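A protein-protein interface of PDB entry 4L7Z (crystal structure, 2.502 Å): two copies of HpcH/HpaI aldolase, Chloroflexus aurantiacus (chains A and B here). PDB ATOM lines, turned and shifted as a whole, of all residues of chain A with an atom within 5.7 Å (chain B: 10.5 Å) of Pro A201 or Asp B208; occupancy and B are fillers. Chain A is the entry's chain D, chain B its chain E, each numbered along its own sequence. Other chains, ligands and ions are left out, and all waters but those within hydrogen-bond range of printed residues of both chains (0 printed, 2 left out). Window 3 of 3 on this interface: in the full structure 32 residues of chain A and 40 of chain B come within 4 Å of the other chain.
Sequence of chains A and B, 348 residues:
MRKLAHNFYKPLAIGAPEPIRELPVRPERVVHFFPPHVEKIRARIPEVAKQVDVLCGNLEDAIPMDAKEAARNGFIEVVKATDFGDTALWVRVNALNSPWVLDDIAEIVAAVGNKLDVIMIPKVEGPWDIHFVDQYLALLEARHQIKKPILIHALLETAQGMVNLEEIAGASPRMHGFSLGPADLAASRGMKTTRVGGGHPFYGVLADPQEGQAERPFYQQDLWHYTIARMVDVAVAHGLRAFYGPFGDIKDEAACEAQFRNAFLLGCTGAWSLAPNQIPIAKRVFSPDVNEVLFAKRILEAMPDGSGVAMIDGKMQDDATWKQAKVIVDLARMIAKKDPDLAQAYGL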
ATOM      1  N   THR A 194       1.908 -18.206  -1.685  1.00  0.00           N
ATOM      2  CA  THR A 194       0.652 -17.532  -1.401  1.00  0.00           C
ATOM      3  C   THR A 194       0.503 -16.333  -2.324  1.00  0.00           C
ATOM      4  O   THR A 194       1.461 -15.938  -2.988  1.00  0.00           O
ATOM      5  CB  THR A 194       0.599 -17.036   0.052  1.00  0.00           C
ATOM      6  OG1 THR A 194       1.648 -16.083   0.269  1.00  0.00           O
ATOM      7  CG2 THR A 194       0.767 -18.196   1.020  1.00  0.00           C
ATOM      8  N   ARG A 195      -0.702 -15.769  -2.358  1.00  0.00           N
ATOM      9  CA  ARG A 195      -0.976 -14.523  -3.073  1.00  0.00           C
ATOM     10  C   ARG A 195      -0.438 -14.525  -4.504  1.00  0.00           C
ATOM     11  O   ARG A 195       0.357 -13.658  -4.871  1.00  0.00           O
ATOM     12  CB  ARG A 195      -0.393 -13.334  -2.306  1.00  0.00           C
ATOM     13  CG  ARG A 195      -0.411 -13.487  -0.788  1.00  0.00           C
ATOM     14  CD  ARG A 195      -1.821 -13.483  -0.222  1.00  0.00           C
ATOM     15  NE  ARG A 195      -1.805 -13.272   1.224  1.00  0.00           N
ATOM     16  CZ  ARG A 195      -1.731 -12.075   1.798  1.00  0.00           C
ATOM     17  NH1 ARG A 195      -1.718 -11.969   3.120  1.00  0.00           N
ATOM     18  NH2 ARG A 195      -1.672 -10.981   1.050  1.00  0.00           N
ATOM     19  N   GLY A 199       5.695 -15.539  -2.142  1.00  0.00           N
ATOM     20  CA  GLY A 199       6.090 -15.905  -0.793  1.00  0.00           C
ATOM     21  C   GLY A 199       5.170 -16.854  -0.049  1.00  0.00           C
ATOM     22  O   GLY A 199       4.097 -17.220  -0.532  1.00  0.00           O
ATOM     23  N   HIS A 200       5.611 -17.255   1.139  1.00  0.00           N
ATOM     24  CA  HIS A 200       4.833 -18.110   2.025  1.00  0.00           C
ATOM     25  C   HIS A 200       5.318 -17.898   3.456  1.00  0.00           C
ATOM     26  O   HIS A 200       6.494 -18.113   3.753  1.00  0.00           O
ATOM     27  CB  HIS A 200       4.983 -19.580   1.629  1.00  0.00           C
ATOM     28  CG  HIS A 200       3.958 -20.480   2.247  1.00  0.00           C
ATOM     29  ND1 HIS A 200       3.985 -20.838   3.577  1.00  0.00           N
ATOM     30  CD2 HIS A 200       2.875 -21.096   1.713  1.00  0.00           C
ATOM     31  CE1 HIS A 200       2.963 -21.635   3.837  1.00  0.00           C
ATOM     32  NE2 HIS A 200       2.275 -21.808   2.724  1.00  0.00           N
ATOM     33  N   PRO A 201       4.408 -17.479   4.351  1.00  0.00           N
ATOM     34  CA  PRO A 201       4.741 -17.090   5.728  1.00  0.00           C
ATOM     35  C   PRO A 201       5.297 -18.230   6.583  1.00  0.00           C
ATOM     36  O   PRO A 201       5.720 -17.988   7.714  1.00  0.00           O
ATOM     37  CB  PRO A 201       3.395 -16.619   6.291  1.00  0.00           C
ATOM     38  CG  PRO A 201       2.375 -17.322   5.468  1.00  0.00           C
ATOM     39  CD  PRO A 201       2.961 -17.393   4.091  1.00  0.00           C
ATOM     40  N   PHE A 202       5.296 -19.448   6.054  1.00  0.00           N
ATOM     41  CA  PHE A 202       5.786 -20.596   6.808  1.00  0.00           C
ATOM     42  C   PHE A 202       7.153 -21.081   6.332  1.00  0.00           C
ATOM     43  O   PHE A 202       7.678 -22.070   6.844  1.00  0.00           O
ATOM     44  CB  PHE A 202       4.766 -21.736   6.783  1.00  0.00           C
ATOM     45  CG  PHE A 202       3.541 -21.465   7.607  1.00  0.00           C
ATOM     46  CD1 PHE A 202       3.462 -21.905   8.918  1.00  0.00           C
ATOM     47  CD2 PHE A 202       2.472 -20.764   7.075  1.00  0.00           C
ATOM     48  CE1 PHE A 202       2.338 -21.655   9.681  1.00  0.00           C
ATOM     49  CE2 PHE A 202       1.344 -20.511   7.833  1.00  0.00           C
ATOM     50  CZ  PHE A 202       1.278 -20.957   9.138  1.00  0.00           C
ATOM     51  N   TYR A 203       7.726 -20.390   5.352  1.00  0.00           N
ATOM     52  CA  TYR A 203       9.096 -20.675   4.939  1.00  0.00           C
ATOM     53  C   TYR A 203      10.071 -19.802   5.718  1.00  0.00           C
ATOM     54  O   TYR A 203      10.292 -18.641   5.375  1.00  0.00           O
ATOM     55  CB  TYR A 203       9.287 -20.465   3.436  1.00  0.00           C
ATOM     56  CG  TYR A 203      10.719 -20.666   2.982  1.00  0.00           C
ATOM     57  CD1 TYR A 203      11.377 -21.867   3.213  1.00  0.00           C
ATOM     58  CD2 TYR A 203      11.410 -19.658   2.324  1.00  0.00           C
ATOM     59  CE1 TYR A 203      12.685 -22.059   2.803  1.00  0.00           C
ATOM     60  CE2 TYR A 203      12.716 -19.843   1.904  1.00  0.00           C
ATOM     61  CZ  TYR A 203      13.349 -21.042   2.149  1.00  0.00           C
ATOM     62  OH  TYR A 203      14.650 -21.228   1.737  1.00  0.00           O
ATOM     63  N   GLY A 204      10.649 -20.367   6.771  1.00  0.00           N
ATOM     64  CA  GLY A 204      11.568 -19.621   7.605  1.00  0.00           C
ATOM     65  C   GLY A 204      12.412 -20.489   8.515  1.00  0.00           C
ATOM     66  O   GLY A 204      12.305 -21.716   8.501  1.00  0.00           O
ATOM     67  N   PHE A 218      10.948 -16.918  14.702  1.00  0.00           N
ATOM     68  CA  PHE A 218      10.805 -17.534  13.392  1.00  0.00           C
ATOM     69  C   PHE A 218      11.098 -16.503  12.310  1.00  0.00           C
ATOM     70  O   PHE A 218      10.317 -15.576  12.096  1.00  0.00           O
ATOM     71  CB  PHE A 218       9.395 -18.101  13.225  1.00  0.00           C
ATOM     72  CG  PHE A 218       9.208 -18.908  11.974  1.00  0.00           C
ATOM     73  CD1 PHE A 218       9.575 -20.243  11.936  1.00  0.00           C
ATOM     74  CD2 PHE A 218       8.658 -18.337  10.839  1.00  0.00           C
ATOM     75  CE1 PHE A 218       9.403 -20.991  10.787  1.00  0.00           C
ATOM     76  CE2 PHE A 218       8.484 -19.078   9.687  1.00  0.00           C
ATOM     77  CZ  PHE A 218       8.855 -20.409   9.662  1.00  0.00           C
ATOM     78  N   GLN A 220      11.309 -15.461   8.650  1.00  0.00           N
ATOM     79  CA  GLN A 220      10.889 -15.752   7.283  1.00  0.00           C
ATOM     80  C   GLN A 220      12.041 -15.591   6.298  1.00  0.00           C
ATOM     81  O   GLN A 220      12.901 -14.728   6.470  1.00  0.00           O
ATOM     82  CB  GLN A 220       9.729 -14.848   6.858  1.00  0.00           C
ATOM     83  CG  GLN A 220       8.413 -15.137   7.553  1.00  0.00           C
ATOM     84  CD  GLN A 220       7.238 -14.482   6.854  1.00  0.00           C
ATOM     85  OE1 GLN A 220       7.237 -14.328   5.632  1.00  0.00           O
ATOM     86  NE2 GLN A 220       6.234 -14.090   7.626  1.00  0.00           N
ATOM     87  N   GLY B 204      14.661  -7.829   1.932  1.00  0.00           N
ATOM     88  CA  GLY B 204      14.026  -8.660   2.934  1.00  0.00           C
ATOM     89  C   GLY B 204      12.598  -9.047   2.613  1.00  0.00           C
ATOM     90  O   GLY B 204      12.027  -8.605   1.617  1.00  0.00           O
ATOM     91  N   VAL B 205      12.021  -9.877   3.474  1.00  0.00           N
ATOM     92  CA  VAL B 205      10.671 -10.383   3.269  1.00  0.00           C
ATOM     93  C   VAL B 205       9.671  -9.669   4.167  1.00  0.00           C
ATOM     94  O   VAL B 205       9.810  -9.668   5.390  1.00  0.00           O
ATOM     95  CB  VAL B 205      10.597 -11.894   3.547  1.00  0.00           C
ATOM     96  CG1 VAL B 205       9.188 -12.414   3.289  1.00  0.00           C
ATOM     97  CG2 VAL B 205      11.609 -12.635   2.693  1.00  0.00           C
ATOM     98  N   LEU B 206       8.664  -9.059   3.551  1.00  0.00           N
ATOM     99  CA  LEU B 206       7.596  -8.410   4.297  1.00  0.00           C
ATOM    100  C   LEU B 206       6.582  -9.454   4.740  1.00  0.00           C
ATOM    101  O   LEU B 206       6.094 -10.238   3.927  1.00  0.00           O
ATOM    102  CB  LEU B 206       6.912  -7.344   3.442  1.00  0.00           C
ATOM    103  CG  LEU B 206       5.860  -6.485   4.146  1.00  0.00           C
ATOM    104  CD1 LEU B 206       6.495  -5.658   5.253  1.00  0.00           C
ATOM    105  CD2 LEU B 206       5.140  -5.589   3.151  1.00  0.00           C
ATOM    106  N   ALA B 207       6.273  -9.468   6.032  1.00  0.00           N
ATOM    107  CA  ALA B 207       5.313 -10.425   6.570  1.00  0.00           C
ATOM    108  C   ALA B 207       3.888 -10.093   6.132  1.00  0.00           C
ATOM    109  O   ALA B 207       3.599  -8.964   5.730  1.00  0.00           O
ATOM    110  CB  ALA B 207       5.411 -10.479   8.085  1.00  0.00           C
ATOM    111  N   ASP B 208       3.007 -11.085   6.206  1.00  0.00           N
ATOM    112  CA  ASP B 208       1.609 -10.904   5.840  1.00  0.00           C
ATOM    113  C   ASP B 208       0.908  -9.952   6.814  1.00  0.00           C
ATOM    114  O   ASP B 208       1.337  -9.823   7.960  1.00  0.00           O
ATOM    115  CB  ASP B 208       0.897 -12.263   5.795  1.00  0.00           C
ATOM    116  CG  ASP B 208       1.359 -13.125   4.634  1.00  0.00           C
ATOM    117  OD1 ASP B 208       1.950 -12.576   3.683  1.00  0.00           O
ATOM    118  OD2 ASP B 208       1.122 -14.352   4.671  1.00  0.00           O
ATOM    119  N   PRO B 209      -0.158  -9.269   6.351  1.00  0.00           N
ATOM    120  CA  PRO B 209      -0.941  -8.315   7.151  1.00  0.00           C
ATOM    121  C   PRO B 209      -1.307  -8.825   8.545  1.00  0.00           C
ATOM    122  O   PRO B 209      -1.920  -9.887   8.654  1.00  0.00           O
ATOM    123  CB  PRO B 209      -2.210  -8.136   6.318  1.00  0.00           C
ATOM    124  CG  PRO B 209      -1.744  -8.294   4.919  1.00  0.00           C
ATOM    125  CD  PRO B 209      -0.635  -9.319   4.955  1.00  0.00           C
ATOM    126  N   GLU B 215       1.514  -3.740  12.900  1.00  0.00           N
ATOM    127  CA  GLU B 215       2.510  -3.491  11.865  1.00  0.00           C
ATOM    128  C   GLU B 215       3.093  -4.798  11.333  1.00  0.00           C
ATOM    129  O   GLU B 215       3.193  -5.786  12.061  1.00  0.00           O
ATOM    130  CB  GLU B 215       3.629  -2.591  12.400  1.00  0.00           C
ATOM    131  CG  GLU B 215       4.648  -2.156  11.350  1.00  0.00           C
ATOM    132  CD  GLU B 215       5.906  -1.573  11.967  1.00  0.00           C
ATOM    133  OE1 GLU B 215       5.805  -0.951  13.047  1.00  0.00           O
ATOM    134  OE2 GLU B 215       6.994  -1.741  11.375  1.00  0.00           O
ATOM    135  N   ARG B 216       3.470  -4.796  10.058  1.00  0.00           N
ATOM    136  CA  ARG B 216       4.040  -5.976   9.425  1.00  0.00           C
ATOM    137  C   ARG B 216       5.558  -6.015   9.574  1.00  0.00           C
ATOM    138  O   ARG B 216       6.253  -5.096   9.140  1.00  0.00           O
ATOM    139  CB  ARG B 216       3.645  -6.018   7.949  1.00  0.00           C
ATOM    140  CG  ARG B 216       2.148  -6.101   7.741  1.00  0.00           C
ATOM    141  CD  ARG B 216       1.756  -5.773   6.314  1.00  0.00           C
ATOM    142  NE  ARG B 216       2.128  -6.827   5.378  1.00  0.00           N
ATOM    143  CZ  ARG B 216       1.799  -6.826   4.091  1.00  0.00           C
ATOM    144  NH1 ARG B 216       1.088  -5.824   3.589  1.00  0.00           N
ATOM    145  NH2 ARG B 216       2.175  -7.824   3.305  1.00  0.00           N
ATOM    146  N   PRO B 217       6.073  -7.084  10.201  1.00  0.00           N
ATOM    147  CA  PRO B 217       7.513  -7.295  10.393  1.00  0.00           C
ATOM    148  C   PRO B 217       8.263  -7.375   9.063  1.00  0.00           C
ATOM    149  O   PRO B 217       7.669  -7.730   8.043  1.00  0.00           O
ATOM    150  CB  PRO B 217       7.572  -8.649  11.110  1.00  0.00           C
ATOM    151  CG  PRO B 217       6.243  -8.790  11.771  1.00  0.00           C
ATOM    152  CD  PRO B 217       5.269  -8.138  10.842  1.00  0.00           C
ATOM    153  N   PHE B 218       9.551  -7.049   9.081  1.00  0.00           N
ATOM    154  CA  PHE B 218      10.373  -7.103   7.878  1.00  0.00           C
ATOM    155  C   PHE B 218      11.686  -7.827   8.163  1.00  0.00           C
ATOM    156  O   PHE B 218      12.538  -7.319   8.897  1.00  0.00           O
ATOM    157  CB  PHE B 218      10.644  -5.690   7.361  1.00  0.00           C
ATOM    158  CG  PHE B 218      11.245  -5.647   5.988  1.00  0.00           C
ATOM    159  CD1 PHE B 218      10.440  -5.733   4.861  1.00  0.00           C
ATOM    160  CD2 PHE B 218      12.612  -5.502   5.821  1.00  0.00           C
ATOM    161  CE1 PHE B 218      10.988  -5.685   3.592  1.00  0.00           C
ATOM    162  CE2 PHE B 218      13.171  -5.454   4.559  1.00  0.00           C
ATOM    163  CZ  PHE B 218      12.358  -5.543   3.438  1.00  0.00           C
ATOM    164  N   TYR B 219      11.840  -9.016   7.584  1.00  0.00           N
ATOM    165  CA  TYR B 219      13.003  -9.861   7.842  1.00  0.00           C
ATOM    166  C   TYR B 219      14.069  -9.681   6.767  1.00  0.00           C
ATOM    167  O   TYR B 219      13.883 -10.109   5.628  1.00  0.00           O
ATOM    168  CB  TYR B 219      12.585 -11.333   7.886  1.00  0.00           C
ATOM    169  CG  TYR B 219      11.417 -11.626   8.802  1.00  0.00           C
ATOM    170  CD1 TYR B 219      11.621 -11.960  10.135  1.00  0.00           C
ATOM    171  CD2 TYR B 219      10.111 -11.583   8.330  1.00  0.00           C
ATOM    172  CE1 TYR B 219      10.556 -12.234  10.974  1.00  0.00           C
ATOM    173  CE2 TYR B 219       9.042 -11.855   9.160  1.00  0.00           C
ATOM    174  CZ  TYR B 219       9.269 -12.179  10.481  1.00  0.00           C
ATOM    175  OH  TYR B 219       8.206 -12.450  11.311  1.00  0.00           O
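Positions printed for both chains: 204 and 218.
Of the 11 printed residues of chain B, 5 touch a printed residue of chain A. Hydrophobic or aromatic side chains of chain B within 4 Å of the printed part of chain A: Val B205, Ala B207, Pro B209 and Tyr B219. Along chain B the printed residues that touch a printed residue of chain A span positions 205 to 219. Printed residues of chain A that touch a printed residue of chain B: Arg A195, Pro A201, Phe A218 and Gln A220. Hydrophobic or aromatic side chains of chain A that line the printed part of chain B: Pro A201. Among the printed residues, 7 pairs touch across the chains. Among the printed residues, Asp or Glu carboxylates within 4 Å of a Lys or Arg side-chain nitrogen of the other chain: Arg A195 with Asp B208 (3.8 Å).
Arg A195 touches Pro B209 (NH1 to CD, 3.4 Å). Pro A201 touches Asp B208 (CG to OD2, 3.3 Å). O of Phe A218 touches CE1 of Tyr B219, at 3.5 Å. Gln A220 touches Val B205. Gln A220 touches Ala B207. Tyr B219 touches Gln A220 (CD2 to CB, 3.6 Å).
Of chain B, only Asp B208 (3.3 Å) comes within 4 Å of Pro A201. Asp B208 touches just these residues of chain A: Arg A195 (3.6 Å) and Pro A201 (3.3 Å). No residue of chain B comes within 4 Å of Phe A202. Printed residues of chain B within 4 Å of Arg A195: Asp B208 and Pro B209. Printed residues of chain A within 4 Å of Pro B209: Arg A195. Gly A204 touches none of the printed residues of chain B. Gly B204 touches none of the printed residues of chain A. The nearest residue of chain B that does not touch Pro A201 is Ala B207 (6.5 Å). The nearest printed residue of chain A that does not touch Tyr B219 is Pro A201 (7.1 Å).
The backbone NH (N) of Val B205 lies within hydrogen-bond range of the backbone carbonyl oxygen (O) of Tyr B219 (2.9 Å). The backbone carbonyl oxygen (O) of Ala B207 lies within hydrogen-bond range of the guanidinium group (NE) of Arg B216 (2.6 Å). The backbone NH of Ala B207 sits at hydrogen-bond distance from the backbone carbonyl oxygen of Pro B217.
The guanidinium group of Arg A195 is in salt-bridge range of the side-chain carboxylate of Asp B208, at 3.8 Å.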
